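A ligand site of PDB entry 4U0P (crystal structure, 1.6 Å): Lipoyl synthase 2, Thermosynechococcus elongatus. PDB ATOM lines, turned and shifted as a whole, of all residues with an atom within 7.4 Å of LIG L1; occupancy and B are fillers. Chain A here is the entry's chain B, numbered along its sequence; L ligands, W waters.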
ATOM      1  N   ILE A  36      27.613 -29.498 -11.649  1.00  0.00           N
ATOM      2  CA  ILE A  36      26.833 -30.398 -12.497  1.00  0.00           C
ATOM      3  C   ILE A  36      26.110 -31.410 -11.610  1.00  0.00           C
ATOM      4  O   ILE A  36      24.954 -31.821 -11.919  1.00  0.00           O
ATOM      5  CB  ILE A  36      27.771 -31.102 -13.490  1.00  0.00           C
ATOM      6  CG1 ILE A  36      28.323 -30.041 -14.457  1.00  0.00           C
ATOM      7  CG2 ILE A  36      27.050 -32.243 -14.206  1.00  0.00           C
ATOM      8  CD1 ILE A  36      27.299 -29.379 -15.354  1.00  0.00           C
ATOM      9  N   LEU A  57      30.469 -26.185 -12.575  1.00  0.00           N
ATOM     10  CA  LEU A  57      30.075 -25.578 -13.851  1.00  0.00           C
ATOM     11  C   LEU A  57      30.426 -24.109 -13.819  1.00  0.00           C
ATOM     12  O   LEU A  57      29.830 -23.334 -13.065  1.00  0.00           O
ATOM     13  CB  LEU A  57      28.570 -25.737 -14.063  1.00  0.00           C
ATOM     14  CG  LEU A  57      27.977 -25.126 -15.321  1.00  0.00           C
ATOM     15  CD1 LEU A  57      28.535 -25.849 -16.455  1.00  0.00           C
ATOM     16  CD2 LEU A  57      26.440 -25.204 -15.261  1.00  0.00           C
ATOM     17  N   THR A  62      23.240 -21.253 -16.728  1.00  0.00           N
ATOM     18  CA  THR A  62      22.486 -21.538 -17.932  1.00  0.00           C
ATOM     19  C   THR A  62      23.361 -21.509 -19.187  1.00  0.00           C
ATOM     20  O   THR A  62      24.470 -20.913 -19.198  1.00  0.00           O
ATOM     21  CB  THR A  62      21.287 -20.574 -18.070  1.00  0.00           C
ATOM     22  OG1 THR A  62      21.755 -19.218 -18.206  1.00  0.00           O
ATOM     23  CG2 THR A  62      20.408 -20.646 -16.833  1.00  0.00           C
ATOM     24  N   CYS A  63      22.916 -22.183 -20.224  1.00  0.00           N
ATOM     25  CA  CYS A  63      23.571 -22.145 -21.531  1.00  0.00           C
ATOM     26  C   CYS A  63      22.564 -21.715 -22.578  1.00  0.00           C
ATOM     27  O   CYS A  63      21.377 -22.083 -22.498  1.00  0.00           O
ATOM     28  CB  CYS A  63      24.183 -23.506 -21.891  1.00  0.00           C
ATOM     29  SG  CYS A  63      25.148 -23.484 -23.421  1.00  0.00           S
ATOM     30  N   THR A  64      23.017 -20.975 -23.574  1.00  0.00           N
ATOM     31  CA  THR A  64      22.100 -20.553 -24.626  1.00  0.00           C
ATOM     32  C   THR A  64      21.934 -21.569 -25.734  1.00  0.00           C
ATOM     33  O   THR A  64      20.995 -21.458 -26.493  1.00  0.00           O
ATOM     34  CB  THR A  64      22.549 -19.225 -25.277  1.00  0.00           C
ATOM     35  OG1 THR A  64      23.816 -19.419 -25.908  1.00  0.00           O
ATOM     36  CG2 THR A  64      22.634 -18.113 -24.216  1.00  0.00           C
ATOM     37  N   ARG A  65      22.821 -22.575 -25.836  1.00  0.00           N
ATOM     38  CA  ARG A  65      22.830 -23.449 -27.017  1.00  0.00           C
ATOM     39  C   ARG A  65      21.679 -24.445 -27.102  1.00  0.00           C
ATOM     40  O   ARG A  65      21.238 -24.798 -28.190  1.00  0.00           O
ATOM     41  CB  ARG A  65      24.125 -24.246 -27.069  1.00  0.00           C
ATOM     42  CG  ARG A  65      25.351 -23.430 -27.342  1.00  0.00           C
ATOM     43  CD  ARG A  65      25.831 -23.646 -28.744  1.00  0.00           C
ATOM     44  NE  ARG A  65      27.130 -23.032 -28.981  1.00  0.00           N
ATOM     45  CZ  ARG A  65      28.272 -23.695 -29.150  1.00  0.00           C
ATOM     46  NH1 ARG A  65      28.296 -25.027 -29.131  1.00  0.00           N
ATOM     47  NH2 ARG A  65      29.394 -23.023 -29.361  1.00  0.00           N
ATOM     48  N   ALA A  66      21.208 -24.935 -25.957  1.00  0.00           N
ATOM     49  CA  ALA A  66      20.091 -25.878 -25.928  1.00  0.00           C
ATOM     50  C   ALA A  66      20.303 -27.175 -26.741  1.00  0.00           C
ATOM     51  O   ALA A  66      19.422 -27.602 -27.505  1.00  0.00           O
ATOM     52  CB  ALA A  66      18.799 -25.188 -26.371  1.00  0.00           C
ATOM     53  N   CYS A  67      21.450 -27.813 -26.557  1.00  0.00           N
ATOM     54  CA  CYS A  67      21.686 -29.130 -27.142  1.00  0.00           C
ATOM     55  C   CYS A  67      20.626 -30.075 -26.640  1.00  0.00           C
ATOM     56  O   CYS A  67      20.234 -30.074 -25.487  1.00  0.00           O
ATOM     57  CB  CYS A  67      23.061 -29.708 -26.792  1.00  0.00           C
ATOM     58  SG  CYS A  67      24.482 -28.627 -27.327  1.00  0.00           S
ATOM     59  N   ALA A  68      20.158 -30.914 -27.554  1.00  0.00           N
ATOM     60  CA  ALA A  68      18.983 -31.706 -27.294  1.00  0.00           C
ATOM     61  C   ALA A  68      19.184 -32.852 -26.313  1.00  0.00           C
ATOM     62  O   ALA A  68      18.214 -33.547 -25.974  1.00  0.00           O
ATOM     63  CB  ALA A  68      18.444 -32.212 -28.604  1.00  0.00           C
ATOM     64  N   PHE A  69      20.424 -33.069 -25.867  1.00  0.00           N
ATOM     65  CA  PHE A  69      20.713 -34.097 -24.845  1.00  0.00           C
ATOM     66  C   PHE A  69      21.057 -33.562 -23.484  1.00  0.00           C
ATOM     67  O   PHE A  69      21.160 -34.308 -22.520  1.00  0.00           O
ATOM     68  CB  PHE A  69      21.878 -34.985 -25.273  1.00  0.00           C
ATOM     69  CG  PHE A  69      23.202 -34.277 -25.243  1.00  0.00           C
ATOM     70  CD1 PHE A  69      23.626 -33.599 -26.345  1.00  0.00           C
ATOM     71  CD2 PHE A  69      23.997 -34.315 -24.112  1.00  0.00           C
ATOM     72  CE1 PHE A  69      24.856 -32.925 -26.328  1.00  0.00           C
ATOM     73  CE2 PHE A  69      25.216 -33.658 -24.085  1.00  0.00           C
ATOM     74  CZ  PHE A  69      25.636 -32.970 -25.195  1.00  0.00           C
ATOM     75  N   CYS A  70      21.282 -32.251 -23.409  1.00  0.00           N
ATOM     76  CA  CYS A  70      21.963 -31.672 -22.270  1.00  0.00           C
ATOM     77  C   CYS A  70      21.047 -31.228 -21.148  1.00  0.00           C
ATOM     78  O   CYS A  70      20.005 -30.612 -21.378  1.00  0.00           O
ATOM     79  CB  CYS A  70      22.768 -30.495 -22.764  1.00  0.00           C
ATOM     80  SG  CYS A  70      23.754 -29.681 -21.487  1.00  0.00           S
ATOM     81  N   GLN A  71      21.482 -31.512 -19.917  1.00  0.00           N
ATOM     82  CA  GLN A  71      20.730 -31.221 -18.713  1.00  0.00           C
ATOM     83  C   GLN A  71      20.873 -29.814 -18.158  1.00  0.00           C
ATOM     84  O   GLN A  71      20.152 -29.438 -17.255  1.00  0.00           O
ATOM     85  CB  GLN A  71      21.126 -32.213 -17.594  1.00  0.00           C
ATOM     86  CG  GLN A  71      22.587 -32.141 -17.151  1.00  0.00           C
ATOM     87  CD  GLN A  71      23.000 -33.365 -16.310  1.00  0.00           C
ATOM     88  OE1 GLN A  71      22.154 -34.126 -15.809  1.00  0.00           O
ATOM     89  NE2 GLN A  71      24.314 -33.577 -16.189  1.00  0.00           N
ATOM     90  N   VAL A  72      21.798 -29.043 -18.722  1.00  0.00           N
ATOM     91  CA  VAL A  72      22.002 -27.652 -18.255  1.00  0.00           C
ATOM     92  C   VAL A  72      20.779 -26.818 -18.608  1.00  0.00           C
ATOM     93  O   VAL A  72      20.212 -26.979 -19.685  1.00  0.00           O
ATOM     94  CB  VAL A  72      23.255 -27.072 -18.920  1.00  0.00           C
ATOM     95  CG1 VAL A  72      23.387 -25.555 -18.631  1.00  0.00           C
ATOM     96  CG2 VAL A  72      24.476 -27.836 -18.431  1.00  0.00           C
ATOM     97  N   GLU A  73      20.347 -25.973 -17.671  1.00  0.00           N
ATOM     98  CA  GLU A  73      19.164 -25.151 -17.862  1.00  0.00           C
ATOM     99  C   GLU A  73      19.384 -24.199 -19.034  1.00  0.00           C
ATOM    100  O   GLU A  73      20.454 -23.571 -19.195  1.00  0.00           O
ATOM    101  CB  GLU A  73      18.828 -24.360 -16.598  1.00  0.00           C
ATOM    102  CG  GLU A  73      17.573 -23.482 -16.705  1.00  0.00           C
ATOM    103  CD  GLU A  73      17.188 -22.804 -15.386  1.00  0.00           C
ATOM    104  OE1 GLU A  73      17.852 -23.065 -14.348  1.00  0.00           O
ATOM    105  OE2 GLU A  73      16.222 -21.995 -15.374  1.00  0.00           O
ATOM    106  N   LYS A  74      18.370 -24.076 -19.869  1.00  0.00           N
ATOM    107  CA  LYS A  74      18.464 -23.208 -21.012  1.00  0.00           C
ATOM    108  C   LYS A  74      18.261 -21.769 -20.562  1.00  0.00           C
ATOM    109  O   LYS A  74      17.439 -21.474 -19.680  1.00  0.00           O
ATOM    110  CB  LYS A  74      17.423 -23.609 -22.047  1.00  0.00           C
ATOM    111  CG  LYS A  74      17.533 -22.846 -23.331  1.00  0.00           C
ATOM    112  CD  LYS A  74      16.437 -23.276 -24.281  1.00  0.00           C
ATOM    113  CE  LYS A  74      16.337 -22.341 -25.477  1.00  0.00           C
ATOM    114  NZ  LYS A  74      15.009 -22.466 -26.128  1.00  0.00           N
ATOM    115  N   THR A 104      34.130 -27.723 -15.591  1.00  0.00           N
ATOM    116  CA  THR A 104      33.534 -27.671 -16.934  1.00  0.00           C
ATOM    117  C   THR A 104      32.850 -26.332 -17.108  1.00  0.00           C
ATOM    118  O   THR A 104      32.820 -25.527 -16.190  1.00  0.00           O
ATOM    119  CB  THR A 104      32.574 -28.850 -17.163  1.00  0.00           C
ATOM    120  OG1 THR A 104      32.254 -28.941 -18.559  1.00  0.00           O
ATOM    121  CG2 THR A 104      31.294 -28.695 -16.371  1.00  0.00           C
ATOM    122  N   SER A 105      32.323 -26.042 -18.284  1.00  0.00           N
ATOM    123  CA  SER A 105      31.625 -24.798 -18.491  1.00  0.00           C
ATOM    124  C   SER A 105      30.569 -24.980 -19.538  1.00  0.00           C
ATOM    125  O   SER A 105      30.509 -25.998 -20.203  1.00  0.00           O
ATOM    126  CB  SER A 105      32.592 -23.720 -18.943  1.00  0.00           C
ATOM    127  OG  SER A 105      33.017 -23.947 -20.248  1.00  0.00           O
ATOM    128  N   VAL A 106      29.680 -23.996 -19.618  1.00  0.00           N
ATOM    129  CA  VAL A 106      28.733 -23.916 -20.723  1.00  0.00           C
ATOM    130  C   VAL A 106      29.473 -23.302 -21.923  1.00  0.00           C
ATOM    131  O   VAL A 106      30.566 -22.750 -21.765  1.00  0.00           O
ATOM    132  CB  VAL A 106      27.497 -23.065 -20.351  1.00  0.00           C
ATOM    133  CG1 VAL A 106      26.859 -23.539 -19.063  1.00  0.00           C
ATOM    134  CG2 VAL A 106      27.898 -21.647 -20.140  1.00  0.00           C
ATOM    135  N   ALA A 107      28.922 -23.421 -23.118  1.00  0.00           N
ATOM    136  CA  ALA A 107      29.532 -22.768 -24.272  1.00  0.00           C
ATOM    137  C   ALA A 107      29.323 -21.264 -24.139  1.00  0.00           C
ATOM    138  O   ALA A 107      28.216 -20.803 -23.847  1.00  0.00           O
ATOM    139  CB  ALA A 107      28.910 -23.238 -25.530  1.00  0.00           C
ATOM    140  N   ARG A 108      30.390 -20.473 -24.357  1.00  0.00           N
ATOM    141  CA  ARG A 108      30.284 -19.029 -24.311  1.00  0.00           C
ATOM    142  C   ARG A 108      30.764 -18.396 -25.612  1.00  0.00           C
ATOM    143  O   ARG A 108      31.861 -17.816 -25.678  1.00  0.00           O
ATOM    144  CB  ARG A 108      31.077 -18.443 -23.144  1.00  0.00           C
ATOM    145  CG  ARG A 108      30.557 -18.899 -21.778  1.00  0.00           C
ATOM    146  CD  ARG A 108      29.146 -18.394 -21.487  1.00  0.00           C
ATOM    147  NE  ARG A 108      29.029 -16.931 -21.548  1.00  0.00           N
ATOM    148  CZ  ARG A 108      28.820 -16.109 -20.529  1.00  0.00           C
ATOM    149  NH1 ARG A 108      28.701 -16.533 -19.275  1.00  0.00           N
ATOM    150  NH2 ARG A 108      28.730 -14.806 -20.777  1.00  0.00           N
ATOM    151  N   PRO A 140      34.749 -27.283 -23.283  1.00  0.00           N
ATOM    152  CA  PRO A 140      34.036 -26.950 -24.538  1.00  0.00           C
ATOM    153  C   PRO A 140      34.947 -27.181 -25.736  1.00  0.00           C
ATOM    154  O   PRO A 140      36.146 -27.442 -25.582  1.00  0.00           O
ATOM    155  CB  PRO A 140      33.717 -25.450 -24.392  1.00  0.00           C
ATOM    156  CG  PRO A 140      34.000 -25.139 -22.914  1.00  0.00           C
ATOM    157  CD  PRO A 140      35.064 -26.053 -22.530  1.00  0.00           C
ATOM    158  N   GLU A 171      30.424 -37.320 -27.340  1.00  0.00           N
ATOM    159  CA  GLU A 171      29.023 -37.502 -26.944  1.00  0.00           C
ATOM    160  C   GLU A 171      28.351 -38.585 -27.754  1.00  0.00           C
ATOM    161  O   GLU A 171      27.659 -39.420 -27.183  1.00  0.00           O
ATOM    162  CB  GLU A 171      28.170 -36.240 -27.052  1.00  0.00           C
ATOM    163  CG  GLU A 171      28.655 -35.042 -26.221  1.00  0.00           C
ATOM    164  CD  GLU A 171      28.665 -35.247 -24.724  1.00  0.00           C
ATOM    165  OE1 GLU A 171      29.009 -34.268 -24.000  1.00  0.00           O
ATOM    166  OE2 GLU A 171      28.364 -36.361 -24.236  1.00  0.00           O
ATOM    167  N   VAL A 180      22.211 -34.399 -32.272  1.00  0.00           N
ATOM    168  CA  VAL A 180      22.467 -34.536 -30.852  1.00  0.00           C
ATOM    169  C   VAL A 180      23.078 -33.234 -30.294  1.00  0.00           C
ATOM    170  O   VAL A 180      22.709 -32.790 -29.203  1.00  0.00           O
ATOM    171  CB  VAL A 180      23.381 -35.739 -30.576  1.00  0.00           C
ATOM    172  CG1 VAL A 180      23.771 -35.798 -29.135  1.00  0.00           C
ATOM    173  CG2 VAL A 180      22.625 -37.026 -30.956  1.00  0.00           C
ATOM    174  N   ARG A 181      24.002 -32.648 -31.047  1.00  0.00           N
ATOM    175  CA  ARG A 181      24.806 -31.527 -30.540  1.00  0.00           C
ATOM    176  C   ARG A 181      24.506 -30.293 -31.388  1.00  0.00           C
ATOM    177  O   ARG A 181      24.098 -30.411 -32.520  1.00  0.00           O
ATOM    178  CB  ARG A 181      26.285 -31.852 -30.667  1.00  0.00           C
ATOM    179  CG  ARG A 181      26.685 -33.152 -30.025  1.00  0.00           C
ATOM    180  CD  ARG A 181      28.129 -33.515 -30.296  1.00  0.00           C
ATOM    181  NE  ARG A 181      29.026 -32.839 -29.357  1.00  0.00           N
ATOM    182  CZ  ARG A 181      30.352 -32.737 -29.492  1.00  0.00           C
ATOM    183  NH1 ARG A 181      30.980 -33.186 -30.576  1.00  0.00           N
ATOM    184  NH2 ARG A 181      31.044 -32.105 -28.544  1.00  0.00           N
ATOM    185  N   ARG A 182      24.647 -29.112 -30.835  1.00  0.00           N
ATOM    186  CA  ARG A 182      24.483 -27.907 -31.631  1.00  0.00           C
ATOM    187  C   ARG A 182      25.792 -27.165 -31.610  1.00  0.00           C
ATOM    188  O   ARG A 182      26.408 -27.002 -30.536  1.00  0.00           O
ATOM    189  CB  ARG A 182      23.356 -27.053 -31.081  1.00  0.00           C
HETATM  190 FE1  LIG L   1      27.523 -27.557 -23.823  1.00  0.00          FE
HETATM  191 FE2  LIG L   1      25.118 -28.264 -22.731  1.00  0.00          FE
HETATM  192 FE3  LIG L   1      25.338 -27.812 -25.374  1.00  0.00          FE
HETATM  193 FE4  LIG L   1      25.452 -25.748 -23.654  1.00  0.00          FE
HETATM  194  S1  LIG L   1      23.802 -27.112 -23.976  1.00  0.00           S
HETATM  195  S2  LIG L   1      26.801 -26.202 -25.326  1.00  0.00           S
HETATM  196  S3  LIG L   1      26.470 -26.752 -22.014  1.00  0.00           S
HETATM  197  S4  LIG L   1      26.277 -29.328 -24.231  1.00  0.00           S
HETATM  198  N1  LG2 L   2      28.048 -28.385 -23.025  1.00  0.00           N
HETATM  199  C1  LG2 L   2      29.497 -28.442 -22.790  1.00  0.00           C
HETATM  200  C2  LG2 L   2      30.025 -29.858 -22.479  1.00  0.00           C
HETATM  201  C3  LG2 L   2      30.306 -30.086 -21.060  1.00  0.00           C
HETATM  202  S1  LG2 L   2      28.778 -30.687 -20.349  1.00  0.00           S
HETATM  203  C4  LG2 L   2      30.044 -28.019 -24.076  1.00  0.00           C
HETATM  204  O1  LG2 L   2      30.771 -28.773 -24.732  1.00  0.00           O
HETATM  205  O2  LG2 L   2      29.660 -26.951 -24.470  1.00  0.00           O
HETATM  206  C5  LG2 L   2      28.345 -29.271 -19.321  1.00  0.00           C
HETATM  207  O   HOH W   1      20.972 -27.074 -22.102  1.00  0.00           O
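N of Cys 67 lies close to S1 of LIG L1 (3.6 Å).
The side-chain sulfur (SG) of Cys 67 binds an iron atom (FE3) of LIG L1 (2.3 Å).
FE4 of LIG L1 is bound by SG of Cys 63 (2.3 Å).
The side-chain sulfur of Cys 70 is bound to an iron atom (FE2) of LIG L1, 2.3 Å away.
N1 of LG2 L2 binds FE1 of LIG L1, at 1.3 Å.
The side-chain sulfur (SG) of Cys 67 lies close to the backbone NH (N) of Arg 182, at 3.5 Å.
The side-chain sulfur of Cys 63 sits close to the backbone NH of Ala 107 (3.8 Å).
The side-chain sulfur of Cys 63 lies close to the backbone NH of Arg 65 (3.5 Å).
N of Cys 63 is in hydrogen-bond range of O of Glu 73, 3.0 Å away.
N of Val 72 lies close to SG of Cys 70, 3.4 Å away.
The backbone carbonyl oxygen of Arg 182 sits at hydrogen-bond distance from the guanidinium group of Arg 65, at 3.1 Å.
Arg 65 touches LIG L1 (CG to S2, 3.7 Å).
N of Ala 66 touches S1 of LIG L1, at 3.9 Å.
Phe 69 touches LIG L1 (CZ to S4, 3.8 Å).
Val 106 touches LIG L1.
Ala 107 touches LIG L1.
Of the 25 residues printed, 8 come within 4 Å of LIG L1.
The nearest printed residue that does not touch LIG L1 is Val 72 (4.2 Å).
Water W1 lies within hydrogen-bond range of O of Val 72 and S1 of LIG L1.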
